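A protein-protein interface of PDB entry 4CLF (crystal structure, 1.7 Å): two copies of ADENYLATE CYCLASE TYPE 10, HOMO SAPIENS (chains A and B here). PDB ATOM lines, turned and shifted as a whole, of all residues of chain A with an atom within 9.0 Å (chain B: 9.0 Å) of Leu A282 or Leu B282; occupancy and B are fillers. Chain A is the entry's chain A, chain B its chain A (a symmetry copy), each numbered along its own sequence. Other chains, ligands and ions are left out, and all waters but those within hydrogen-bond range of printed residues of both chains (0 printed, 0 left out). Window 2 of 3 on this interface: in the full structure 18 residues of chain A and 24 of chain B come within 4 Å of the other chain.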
ATOM      1  N   SER A 272      -8.478   9.337 -14.664  1.00  0.00           N
ATOM      2  CA  SER A 272      -9.269   8.129 -14.492  1.00  0.00           C
ATOM      3  C   SER A 272      -8.709   7.204 -13.409  1.00  0.00           C
ATOM      4  O   SER A 272      -9.478   6.484 -12.784  1.00  0.00           O
ATOM      5  CB  SER A 272      -9.335   7.319 -15.796  1.00  0.00           C
ATOM      6  OG  SER A 272      -8.060   7.202 -16.338  1.00  0.00           O
ATOM      7  N   ILE A 273      -7.384   7.210 -13.237  1.00  0.00           N
ATOM      8  CA  ILE A 273      -6.745   6.441 -12.150  1.00  0.00           C
ATOM      9  C   ILE A 273      -7.149   7.027 -10.783  1.00  0.00           C
ATOM     10  O   ILE A 273      -7.508   6.328  -9.851  1.00  0.00           O
ATOM     11  CB  ILE A 273      -5.227   6.403 -12.316  1.00  0.00           C
ATOM     12  CG1 ILE A 273      -4.851   5.589 -13.583  1.00  0.00           C
ATOM     13  CG2 ILE A 273      -4.611   5.825 -11.058  1.00  0.00           C
ATOM     14  CD1 ILE A 273      -4.768   4.153 -13.331  1.00  0.00           C
ATOM     15  N   LYS A 275      -9.849   8.594 -10.171  1.00  0.00           N
ATOM     16  CA  LYS A 275     -11.269   8.272  -9.984  1.00  0.00           C
ATOM     17  C   LYS A 275     -11.376   6.900  -9.295  1.00  0.00           C
ATOM     18  O   LYS A 275     -12.115   6.710  -8.334  1.00  0.00           O
ATOM     19  CB  LYS A 275     -12.016   8.308 -11.313  1.00  0.00           C
ATOM     20  CG  LYS A 275     -13.508   8.366 -11.147  1.00  0.00           C
ATOM     21  CD  LYS A 275     -14.258   8.438 -12.440  1.00  0.00           C
ATOM     22  CE  LYS A 275     -15.745   8.629 -12.128  1.00  0.00           C
ATOM     23  NZ  LYS A 275     -16.476   8.789 -13.434  1.00  0.00           N
ATOM     24  N   GLN A 276     -10.537   5.964  -9.752  1.00  0.00           N
ATOM     25  CA  GLN A 276     -10.532   4.616  -9.111  1.00  0.00           C
ATOM     26  C   GLN A 276     -10.017   4.665  -7.718  1.00  0.00           C
ATOM     27  O   GLN A 276     -10.594   4.065  -6.786  1.00  0.00           O
ATOM     28  CB  GLN A 276      -9.721   3.660 -10.002  1.00  0.00           C
ATOM     29  CG  GLN A 276      -9.675   2.270  -9.548  1.00  0.00           C
ATOM     30  CD  GLN A 276      -8.658   1.466 -10.347  1.00  0.00           C
ATOM     31  OE1 GLN A 276      -8.705   1.454 -11.594  1.00  0.00           O
ATOM     32  NE2 GLN A 276      -7.715   0.859  -9.634  1.00  0.00           N
ATOM     33  N   ILE A 277      -8.966   5.423  -7.516  1.00  0.00           N
ATOM     34  CA  ILE A 277      -8.358   5.618  -6.191  1.00  0.00           C
ATOM     35  C   ILE A 277      -9.358   6.174  -5.186  1.00  0.00           C
ATOM     36  O   ILE A 277      -9.343   5.824  -3.993  1.00  0.00           O
ATOM     37  CB  ILE A 277      -7.090   6.478  -6.317  1.00  0.00           C
ATOM     38  CG1 ILE A 277      -5.928   5.638  -6.898  1.00  0.00           C
ATOM     39  CG2 ILE A 277      -6.699   7.161  -5.001  1.00  0.00           C
ATOM     40  CD1 ILE A 277      -4.718   6.430  -7.223  1.00  0.00           C
ATOM     41  N   ASP A 278     -10.212   7.054  -5.688  1.00  0.00           N
ATOM     42  CA  ASP A 278     -11.248   7.708  -4.848  1.00  0.00           C
ATOM     43  C   ASP A 278     -12.503   6.846  -4.739  1.00  0.00           C
ATOM     44  O   ASP A 278     -13.480   7.265  -4.150  1.00  0.00           O
ATOM     45  CB  ASP A 278     -11.580   9.043  -5.433  1.00  0.00           C
ATOM     46  CG  ASP A 278     -10.439  10.073  -5.230  1.00  0.00           C
ATOM     47  OD1 ASP A 278      -9.769  10.021  -4.181  1.00  0.00           O
ATOM     48  OD2 ASP A 278     -10.320  10.980  -6.114  1.00  0.00           O
ATOM     49  N   ASN A 279     -12.413   5.590  -5.175  1.00  0.00           N
ATOM     50  CA  ASN A 279     -13.572   4.681  -5.134  1.00  0.00           C
ATOM     51  C   ASN A 279     -14.798   5.253  -5.792  1.00  0.00           C
ATOM     52  O   ASN A 279     -15.941   5.005  -5.324  1.00  0.00           O
ATOM     53  CB  ASN A 279     -13.856   4.250  -3.694  1.00  0.00           C
ATOM     54  CG  ASN A 279     -12.720   3.472  -3.062  1.00  0.00           C
ATOM     55  OD1 ASN A 279     -12.048   2.705  -3.695  1.00  0.00           O
ATOM     56  ND2 ASN A 279     -12.470   3.744  -1.829  1.00  0.00           N
ATOM     57  N   LYS A 280     -14.603   5.940  -6.890  1.00  0.00           N
ATOM     58  CA  LYS A 280     -15.645   6.503  -7.743  1.00  0.00           C
ATOM     59  C   LYS A 280     -15.752   5.848  -9.106  1.00  0.00           C
ATOM     60  O   LYS A 280     -16.578   6.180  -9.924  1.00  0.00           O
ATOM     61  CB  LYS A 280     -15.488   8.075  -7.845  1.00  0.00           C
ATOM     62  CG  LYS A 280     -15.912   8.754  -6.507  1.00  0.00           C
ATOM     63  CD  LYS A 280     -15.992  10.310  -6.687  1.00  0.00           C
ATOM     64  CE  LYS A 280     -16.554  11.069  -5.423  1.00  0.00           C
ATOM     65  NZ  LYS A 280     -15.723  10.962  -4.202  1.00  0.00           N
ATOM     66  N   GLN A 281     -14.953   4.768  -9.258  1.00  0.00           N
ATOM     67  CA  GLN A 281     -14.931   3.946 -10.466  1.00  0.00           C
ATOM     68  C   GLN A 281     -14.564   2.521 -10.008  1.00  0.00           C
ATOM     69  O   GLN A 281     -13.761   2.364  -9.084  1.00  0.00           O
ATOM     70  CB  GLN A 281     -13.832   4.476 -11.371  1.00  0.00           C
ATOM     71  CG  GLN A 281     -13.700   3.917 -12.766  1.00  0.00           C
ATOM     72  CD  GLN A 281     -12.862   4.862 -13.632  1.00  0.00           C
ATOM     73  OE1 GLN A 281     -13.410   5.802 -14.179  1.00  0.00           O
ATOM     74  NE2 GLN A 281     -11.562   4.710 -13.641  1.00  0.00           N
ATOM     75  N   LEU A 282     -15.140   1.529 -10.654  1.00  0.00           N
ATOM     76  CA  LEU A 282     -14.810   0.121 -10.317  1.00  0.00           C
ATOM     77  C   LEU A 282     -13.355  -0.197 -10.609  1.00  0.00           C
ATOM     78  O   LEU A 282     -12.754   0.332 -11.504  1.00  0.00           O
ATOM     79  CB  LEU A 282     -15.703  -0.760 -11.207  1.00  0.00           C
ATOM     80  CG  LEU A 282     -17.166  -0.668 -10.866  1.00  0.00           C
ATOM     81  CD1 LEU A 282     -18.017  -1.091 -12.085  1.00  0.00           C
ATOM     82  CD2 LEU A 282     -17.455  -1.443  -9.637  1.00  0.00           C
ATOM     83  N   GLN A 283     -12.785  -1.016  -9.714  1.00  0.00           N
ATOM     84  CA  GLN A 283     -11.327  -1.234  -9.586  1.00  0.00           C
ATOM     85  C   GLN A 283     -10.808  -1.945 -10.765  1.00  0.00           C
ATOM     86  O   GLN A 283      -9.604  -1.828 -11.035  1.00  0.00           O
ATOM     87  CB  GLN A 283     -10.970  -1.954  -8.278  1.00  0.00           C
ATOM     88  CG  GLN A 283     -11.275  -1.106  -7.024  1.00  0.00           C
ATOM     89  CD  GLN A 283     -10.452   0.205  -6.874  1.00  0.00           C
ATOM     90  OE1 GLN A 283      -9.212   0.253  -7.139  1.00  0.00           O
ATOM     91  NE2 GLN A 283     -11.133   1.273  -6.471  1.00  0.00           N
ATOM     92  N   GLY A 284     -11.695  -2.623 -11.512  1.00  0.00           N
ATOM     93  CA  GLY A 284     -11.397  -3.337 -12.720  1.00  0.00           C
ATOM     94  C   GLY A 284     -11.707  -2.670 -14.012  1.00  0.00           C
ATOM     95  O   GLY A 284     -11.403  -3.202 -15.051  1.00  0.00           O
ATOM     96  N   TYR A 285     -12.167  -1.393 -14.005  1.00  0.00           N
ATOM     97  CA  TYR A 285     -12.650  -0.773 -15.201  1.00  0.00           C
ATOM     98  C   TYR A 285     -11.532  -0.384 -16.262  1.00  0.00           C
ATOM     99  O   TYR A 285     -11.763  -0.276 -17.411  1.00  0.00           O
ATOM    100  CB  TYR A 285     -13.309   0.599 -14.793  1.00  0.00           C
ATOM    101  CG  TYR A 285     -13.805   1.501 -15.898  1.00  0.00           C
ATOM    102  CD1 TYR A 285     -15.118   1.428 -16.385  1.00  0.00           C
ATOM    103  CD2 TYR A 285     -12.986   2.531 -16.368  1.00  0.00           C
ATOM    104  CE1 TYR A 285     -15.553   2.349 -17.384  1.00  0.00           C
ATOM    105  CE2 TYR A 285     -13.400   3.428 -17.321  1.00  0.00           C
ATOM    106  CZ  TYR A 285     -14.673   3.340 -17.842  1.00  0.00           C
ATOM    107  OH  TYR A 285     -14.966   4.296 -18.822  1.00  0.00           O
ATOM    108  N   LEU A 286     -10.348  -0.186 -15.780  1.00  0.00           N
ATOM    109  CA  LEU A 286      -9.247   0.249 -16.653  1.00  0.00           C
ATOM    110  C   LEU A 286      -8.506  -0.939 -17.277  1.00  0.00           C
ATOM    111  O   LEU A 286      -7.598  -0.639 -18.118  1.00  0.00           O
ATOM    112  CB  LEU A 286      -8.257   1.143 -15.861  1.00  0.00           C
ATOM    113  CG  LEU A 286      -8.828   2.541 -15.622  1.00  0.00           C
ATOM    114  CD1 LEU A 286      -7.830   3.281 -14.737  1.00  0.00           C
ATOM    115  CD2 LEU A 286      -9.064   3.293 -16.902  1.00  0.00           C
ATOM    116  N   SER A 287      -8.823  -2.189 -16.977  1.00  0.00           N
ATOM    117  CA  SER A 287      -8.201  -3.365 -17.655  1.00  0.00           C
ATOM    118  C   SER A 287      -9.036  -3.656 -18.892  1.00  0.00           C
ATOM    119  O   SER A 287     -10.113  -4.167 -18.754  1.00  0.00           O
ATOM    120  CB  SER A 287      -8.124  -4.577 -16.782  1.00  0.00           C
ATOM    121  OG  SER A 287      -7.233  -4.328 -15.704  1.00  0.00           O
ATOM    122  N   ILE A 395      -3.454  -1.281 -15.275  1.00  0.00           N
ATOM    123  CA  ILE A 395      -2.469  -0.994 -14.238  1.00  0.00           C
ATOM    124  C   ILE A 395      -1.602  -2.232 -14.062  1.00  0.00           C
ATOM    125  O   ILE A 395      -2.107  -3.304 -13.627  1.00  0.00           O
ATOM    126  CB  ILE A 395      -3.181  -0.599 -12.910  1.00  0.00           C
ATOM    127  CG1 ILE A 395      -3.924   0.720 -13.180  1.00  0.00           C
ATOM    128  CG2 ILE A 395      -2.176  -0.456 -11.805  1.00  0.00           C
ATOM    129  CD1 ILE A 395      -4.872   1.139 -12.073  1.00  0.00           C
ATOM    130  N   SER B 272     -29.260   5.937   0.963  1.00  0.00           N
ATOM    131  CA  SER B 272     -28.075   5.895   0.121  1.00  0.00           C
ATOM    132  C   SER B 272     -26.866   5.282   0.832  1.00  0.00           C
ATOM    133  O   SER B 272     -26.020   4.695   0.169  1.00  0.00           O
ATOM    134  CB  SER B 272     -27.669   7.305  -0.335  1.00  0.00           C
ATOM    135  OG  SER B 272     -27.676   8.169   0.755  1.00  0.00           O
ATOM    136  N   ILE B 273     -26.788   5.462   2.154  1.00  0.00           N
ATOM    137  CA  ILE B 273     -25.725   4.824   2.956  1.00  0.00           C
ATOM    138  C   ILE B 273     -25.911   3.293   2.952  1.00  0.00           C
ATOM    139  O   ILE B 273     -24.986   2.522   2.760  1.00  0.00           O
ATOM    140  CB  ILE B 273     -25.694   5.380   4.378  1.00  0.00           C
ATOM    141  CG1 ILE B 273     -25.263   6.869   4.357  1.00  0.00           C
ATOM    142  CG2 ILE B 273     -24.767   4.525   5.219  1.00  0.00           C
ATOM    143  CD1 ILE B 273     -23.812   7.041   4.357  1.00  0.00           C
ATOM    144  N   LYS B 275     -27.312   1.609   0.645  1.00  0.00           N
ATOM    145  CA  LYS B 275     -26.989   1.155  -0.713  1.00  0.00           C
ATOM    146  C   LYS B 275     -25.482   0.855  -0.785  1.00  0.00           C
ATOM    147  O   LYS B 275     -25.046  -0.177  -1.287  1.00  0.00           O
ATOM    148  CB  LYS B 275     -27.419   2.186  -1.750  1.00  0.00           C
ATOM    149  CG  LYS B 275     -27.468   1.632  -3.146  1.00  0.00           C
ATOM    150  CD  LYS B 275     -27.924   2.620  -4.173  1.00  0.00           C
ATOM    151  CE  LYS B 275     -28.059   1.896  -5.516  1.00  0.00           C
ATOM    152  NZ  LYS B 275     -28.601   2.877  -6.520  1.00  0.00           N
ATOM    153  N   GLN B 276     -24.691   1.746  -0.177  1.00  0.00           N
ATOM    154  CA  GLN B 276     -23.216   1.512  -0.150  1.00  0.00           C
ATOM    155  C   GLN B 276     -22.855   0.338   0.686  1.00  0.00           C
ATOM    156  O   GLN B 276     -22.032  -0.516   0.294  1.00  0.00           O
ATOM    157  CB  GLN B 276     -22.531   2.804   0.326  1.00  0.00           C
ATOM    158  CG  GLN B 276     -21.068   2.765   0.342  1.00  0.00           C
ATOM    159  CD  GLN B 276     -20.497   3.984   1.053  1.00  0.00           C
ATOM    160  OE1 GLN B 276     -20.839   5.134   0.707  1.00  0.00           O
ATOM    161  NE2 GLN B 276     -19.687   3.728   2.076  1.00  0.00           N
ATOM    162  N   ILE B 277     -23.496   0.220   1.824  1.00  0.00           N
ATOM    163  CA  ILE B 277     -23.292  -0.906   2.748  1.00  0.00           C
ATOM    164  C   ILE B 277     -23.567  -2.246   2.079  1.00  0.00           C
ATOM    165  O   ILE B 277     -22.893  -3.256   2.346  1.00  0.00           O
ATOM    166  CB  ILE B 277     -24.117  -0.692   4.027  1.00  0.00           C
ATOM    167  CG1 ILE B 277     -23.445   0.372   4.927  1.00  0.00           C
ATOM    168  CG2 ILE B 277     -24.388  -1.995   4.788  1.00  0.00           C
ATOM    169  CD1 ILE B 277     -24.265   0.774   6.096  1.00  0.00           C
ATOM    170  N   ASP B 278     -24.576  -2.235   1.220  1.00  0.00           N
ATOM    171  CA  ASP B 278     -24.992  -3.457   0.486  1.00  0.00           C
ATOM    172  C   ASP B 278     -24.169  -3.652  -0.785  1.00  0.00           C
ATOM    173  O   ASP B 278     -24.429  -4.563  -1.546  1.00  0.00           O
ATOM    174  CB  ASP B 278     -26.447  -3.356   0.156  1.00  0.00           C
ATOM    175  CG  ASP B 278     -27.346  -3.526   1.407  1.00  0.00           C
ATOM    176  OD1 ASP B 278     -26.982  -4.312   2.301  1.00  0.00           O
ATOM    177  OD2 ASP B 278     -28.463  -2.916   1.398  1.00  0.00           O
ATOM    178  N   ASN B 279     -23.085  -2.888  -0.926  1.00  0.00           N
ATOM    179  CA  ASN B 279     -22.234  -2.982  -2.124  1.00  0.00           C
ATOM    180  C   ASN B 279     -23.002  -2.840  -3.410  1.00  0.00           C
ATOM    181  O   ASN B 279     -22.662  -3.504  -4.426  1.00  0.00           O
ATOM    182  CB  ASN B 279     -21.420  -4.277  -2.095  1.00  0.00           C
ATOM    183  CG  ASN B 279     -20.465  -4.364  -0.923  1.00  0.00           C
ATOM    184  OD1 ASN B 279     -19.891  -3.398  -0.501  1.00  0.00           O
ATOM    185  ND2 ASN B 279     -20.370  -5.517  -0.358  1.00  0.00           N
ATOM    186  N   LYS B 280     -23.966  -1.954  -3.419  1.00  0.00           N
ATOM    187  CA  LYS B 280     -24.775  -1.582  -4.574  1.00  0.00           C
ATOM    188  C   LYS B 280     -24.536  -0.169  -5.070  1.00  0.00           C
ATOM    189  O   LYS B 280     -25.109   0.288  -6.031  1.00  0.00           O
ATOM    190  CB  LYS B 280     -26.307  -1.866  -4.293  1.00  0.00           C
ATOM    191  CG  LYS B 280     -26.591  -3.399  -4.315  1.00  0.00           C
ATOM    192  CD  LYS B 280     -28.135  -3.669  -4.283  1.00  0.00           C
ATOM    193  CE  LYS B 280     -28.520  -5.190  -4.447  1.00  0.00           C
ATOM    194  NZ  LYS B 280     -28.050  -6.081  -3.362  1.00  0.00           N
ATOM    195  N   GLN B 281     -23.523   0.467  -4.440  1.00  0.00           N
ATOM    196  CA  GLN B 281     -23.076   1.813  -4.790  1.00  0.00           C
ATOM    197  C   GLN B 281     -21.570   1.864  -4.466  1.00  0.00           C
ATOM    198  O   GLN B 281     -21.137   1.255  -3.483  1.00  0.00           O
ATOM    199  CB  GLN B 281     -23.810   2.796  -3.894  1.00  0.00           C
ATOM    200  CG  GLN B 281     -23.667   4.274  -4.156  1.00  0.00           C
ATOM    201  CD  GLN B 281     -24.795   5.042  -3.463  1.00  0.00           C
ATOM    202  OE1 GLN B 281     -25.867   5.158  -4.031  1.00  0.00           O
ATOM    203  NE2 GLN B 281     -24.617   5.428  -2.224  1.00  0.00           N
ATOM    204  N   LEU B 282     -20.818   2.580  -5.274  1.00  0.00           N
ATOM    205  CA  LEU B 282     -19.364   2.728  -5.012  1.00  0.00           C
ATOM    206  C   LEU B 282     -19.102   3.460  -3.708  1.00  0.00           C
ATOM    207  O   LEU B 282     -19.847   4.305  -3.291  1.00  0.00           O
ATOM    208  CB  LEU B 282     -18.795   3.559  -6.175  1.00  0.00           C
ATOM    209  CG  LEU B 282     -18.826   2.841  -7.497  1.00  0.00           C
ATOM    210  CD1 LEU B 282     -18.789   3.866  -8.653  1.00  0.00           C
ATOM    211  CD2 LEU B 282     -17.743   1.832  -7.557  1.00  0.00           C
ATOM    212  N   GLN B 283     -18.049   2.995  -3.023  1.00  0.00           N
ATOM    213  CA  GLN B 283     -17.764   3.310  -1.606  1.00  0.00           C
ATOM    214  C   GLN B 283     -17.403   4.729  -1.458  1.00  0.00           C
ATOM    215  O   GLN B 283     -17.559   5.259  -0.349  1.00  0.00           O
ATOM    216  CB  GLN B 283     -16.694   2.380  -1.018  1.00  0.00           C
ATOM    217  CG  GLN B 283     -17.160   0.911  -0.927  1.00  0.00           C
ATOM    218  CD  GLN B 283     -18.352   0.633   0.032  1.00  0.00           C
ATOM    219  OE1 GLN B 283     -18.439   1.188   1.170  1.00  0.00           O
ATOM    220  NE2 GLN B 283     -19.280  -0.201  -0.425  1.00  0.00           N
ATOM    221  N   GLY B 284     -16.988   5.375  -2.560  1.00  0.00           N
ATOM    222  CA  GLY B 284     -16.637   6.764  -2.633  1.00  0.00           C
ATOM    223  C   GLY B 284     -17.652   7.705  -3.178  1.00  0.00           C
ATOM    224  O   GLY B 284     -17.428   8.890  -3.185  1.00  0.00           O
ATOM    225  N   TYR B 285     -18.886   7.239  -3.494  1.00  0.00           N
ATOM    226  CA  TYR B 285     -19.832   8.059  -4.187  1.00  0.00           C
ATOM    227  C   TYR B 285     -20.476   9.229  -3.324  1.00  0.00           C
ATOM    228  O   TYR B 285     -20.911  10.208  -3.813  1.00  0.00           O
ATOM    229  CB  TYR B 285     -21.050   7.143  -4.592  1.00  0.00           C
ATOM    230  CG  TYR B 285     -22.241   7.801  -5.247  1.00  0.00           C
ATOM    231  CD1 TYR B 285     -22.345   7.933  -6.639  1.00  0.00           C
ATOM    232  CD2 TYR B 285     -23.340   8.174  -4.467  1.00  0.00           C
ATOM    233  CE1 TYR B 285     -23.522   8.503  -7.210  1.00  0.00           C
ATOM    234  CE2 TYR B 285     -24.480   8.712  -5.009  1.00  0.00           C
ATOM    235  CZ  TYR B 285     -24.578   8.890  -6.372  1.00  0.00           C
ATOM    236  OH  TYR B 285     -25.780   9.470  -6.796  1.00  0.00           O
ATOM    237  N   LEU B 286     -20.497   9.034  -2.046  1.00  0.00           N
ATOM    238  CA  LEU B 286     -21.132  10.013  -1.149  1.00  0.00           C
ATOM    239  C   LEU B 286     -20.150  11.100  -0.700  1.00  0.00           C
ATOM    240  O   LEU B 286     -20.651  12.035   0.004  1.00  0.00           O
ATOM    241  CB  LEU B 286     -21.737   9.294   0.085  1.00  0.00           C
ATOM    242  CG  LEU B 286     -23.026   8.551  -0.273  1.00  0.00           C
ATOM    243  CD1 LEU B 286     -23.457   7.789   0.976  1.00  0.00           C
ATOM    244  CD2 LEU B 286     -24.115   9.478  -0.734  1.00  0.00           C
ATOM    245  N   SER B 287     -18.875  11.074  -1.057  1.00  0.00           N
ATOM    246  CA  SER B 287     -17.922  12.178  -0.735  1.00  0.00           C
ATOM    247  C   SER B 287     -18.017  13.189  -1.866  1.00  0.00           C
ATOM    248  O   SER B 287     -17.516  12.919  -2.924  1.00  0.00           O
ATOM    249  CB  SER B 287     -16.511  11.711  -0.569  1.00  0.00           C
ATOM    250  OG  SER B 287     -16.421  10.873   0.575  1.00  0.00           O
ATOM    251  N   ILE B 395     -19.119  10.637   4.627  1.00  0.00           N
ATOM    252  CA  ILE B 395     -19.074   9.851   5.855  1.00  0.00           C
ATOM    253  C   ILE B 395     -17.814  10.243   6.613  1.00  0.00           C
ATOM    254  O   ILE B 395     -16.676   9.994   6.124  1.00  0.00           O
ATOM    255  CB  ILE B 395     -19.096   8.329   5.526  1.00  0.00           C
ATOM    256  CG1 ILE B 395     -20.456   8.037   4.872  1.00  0.00           C
ATOM    257  CG2 ILE B 395     -18.892   7.525   6.775  1.00  0.00           C
ATOM    258  CD1 ILE B 395     -20.570   6.651   4.263  1.00  0.00           C
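The backbone carbonyl oxygen (O) of Asn A279 lies within hydrogen-bond range of the backbone NH (N) of Gly B284 (3.0 Å).
The side-chain amino group (NZ) of Lys A280 lies within hydrogen-bond range of the backbone carbonyl oxygen (O) of Gly B284 (2.9 Å).
The side-chain amino group of Lys A280 sits at hydrogen-bond distance from the backbone carbonyl oxygen of Ser B287 (2.9 Å).
Hydrophobic or aromatic side chains of chain B within 4 Å of the printed part of chain A: Leu B282.
Hydrophobic or aromatic side chains of chain A within 4 Å of the printed part of chain B: Leu A282.
Among the printed residues, 9 pairs touch across the chains.
Among the printed residues, no Asp or Glu carboxylate lies within 4 Å of a Lys or Arg side-chain nitrogen of the other chain.
Asp A278 touches Gly B284, but with the chains exchanged Gly A284 does not touch Asp B278 (16.3 Å).
Lys A280 touches Leu B282, but with the chains exchanged Leu A282 does not touch Lys B280 (8.5 Å).
Lys A280 touches Ser B287, but with the chains exchanged Ser A287 does not touch Lys B280 (19.8 Å).
Gln A281 touches Leu B282, but with the chains exchanged Leu A282 does not touch Gln B281 (7.4 Å).
Of the 9 pairs that touch across the chains among the printed residues, 1 has its exchanged pair printed and touching as well.
Leu A282 touches one residue of chain B.
Of the printed residues of chain A, Leu B282 touches Asn A279, Lys A280, Gln A281 and Leu A282.
Of the printed residues of chain A, Gln B283 touches Asn A279 (3.7 Å).
Of the printed residues of chain B, Asn A279 touches Leu B282 (3.3 Å), Gln B283 (3.7 Å) and Gly B284 (3.0 Å).
The nearest printed residue of chain B that does not touch Gln A281 is Gly B284 (7.0 Å).
O of Asp A278 touches CA of Gly B284 (3.5 Å).
Leu B282 touches Asn A279.
O of Asn A279 touches N of Gln B283, at 3.7 Å.
Lys A280 touches Leu B282 (O to CD1, 3.4 Å).
Leu B282 touches Gln A281 (CD1 to N, 3.99 Å).
CD2 of Leu A282 touches CD2 of Leu B282, 3.9 Å away.
The side-chain amide nitrogen (NE2) of Gln A281 is in hydrogen-bond range of the backbone carbonyl oxygen (O) of Ser A272 (2.9 Å).
O of Lys A275 sits at hydrogen-bond distance from N of Lys A280 (3.0 Å).
The side-chain amide oxygen (OD1) of Asn A279 lies within hydrogen-bond range of the side-chain amide nitrogen (NE2) of Gln A283, 3.3 Å away.
The side-chain amide nitrogen of Gln B283 lies within hydrogen-bond range of the backbone carbonyl oxygen of Gln B276 (2.9 Å).
OD1 of Asn B279 sits at hydrogen-bond distance from NE2 of Gln B283, at 3.3 Å.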
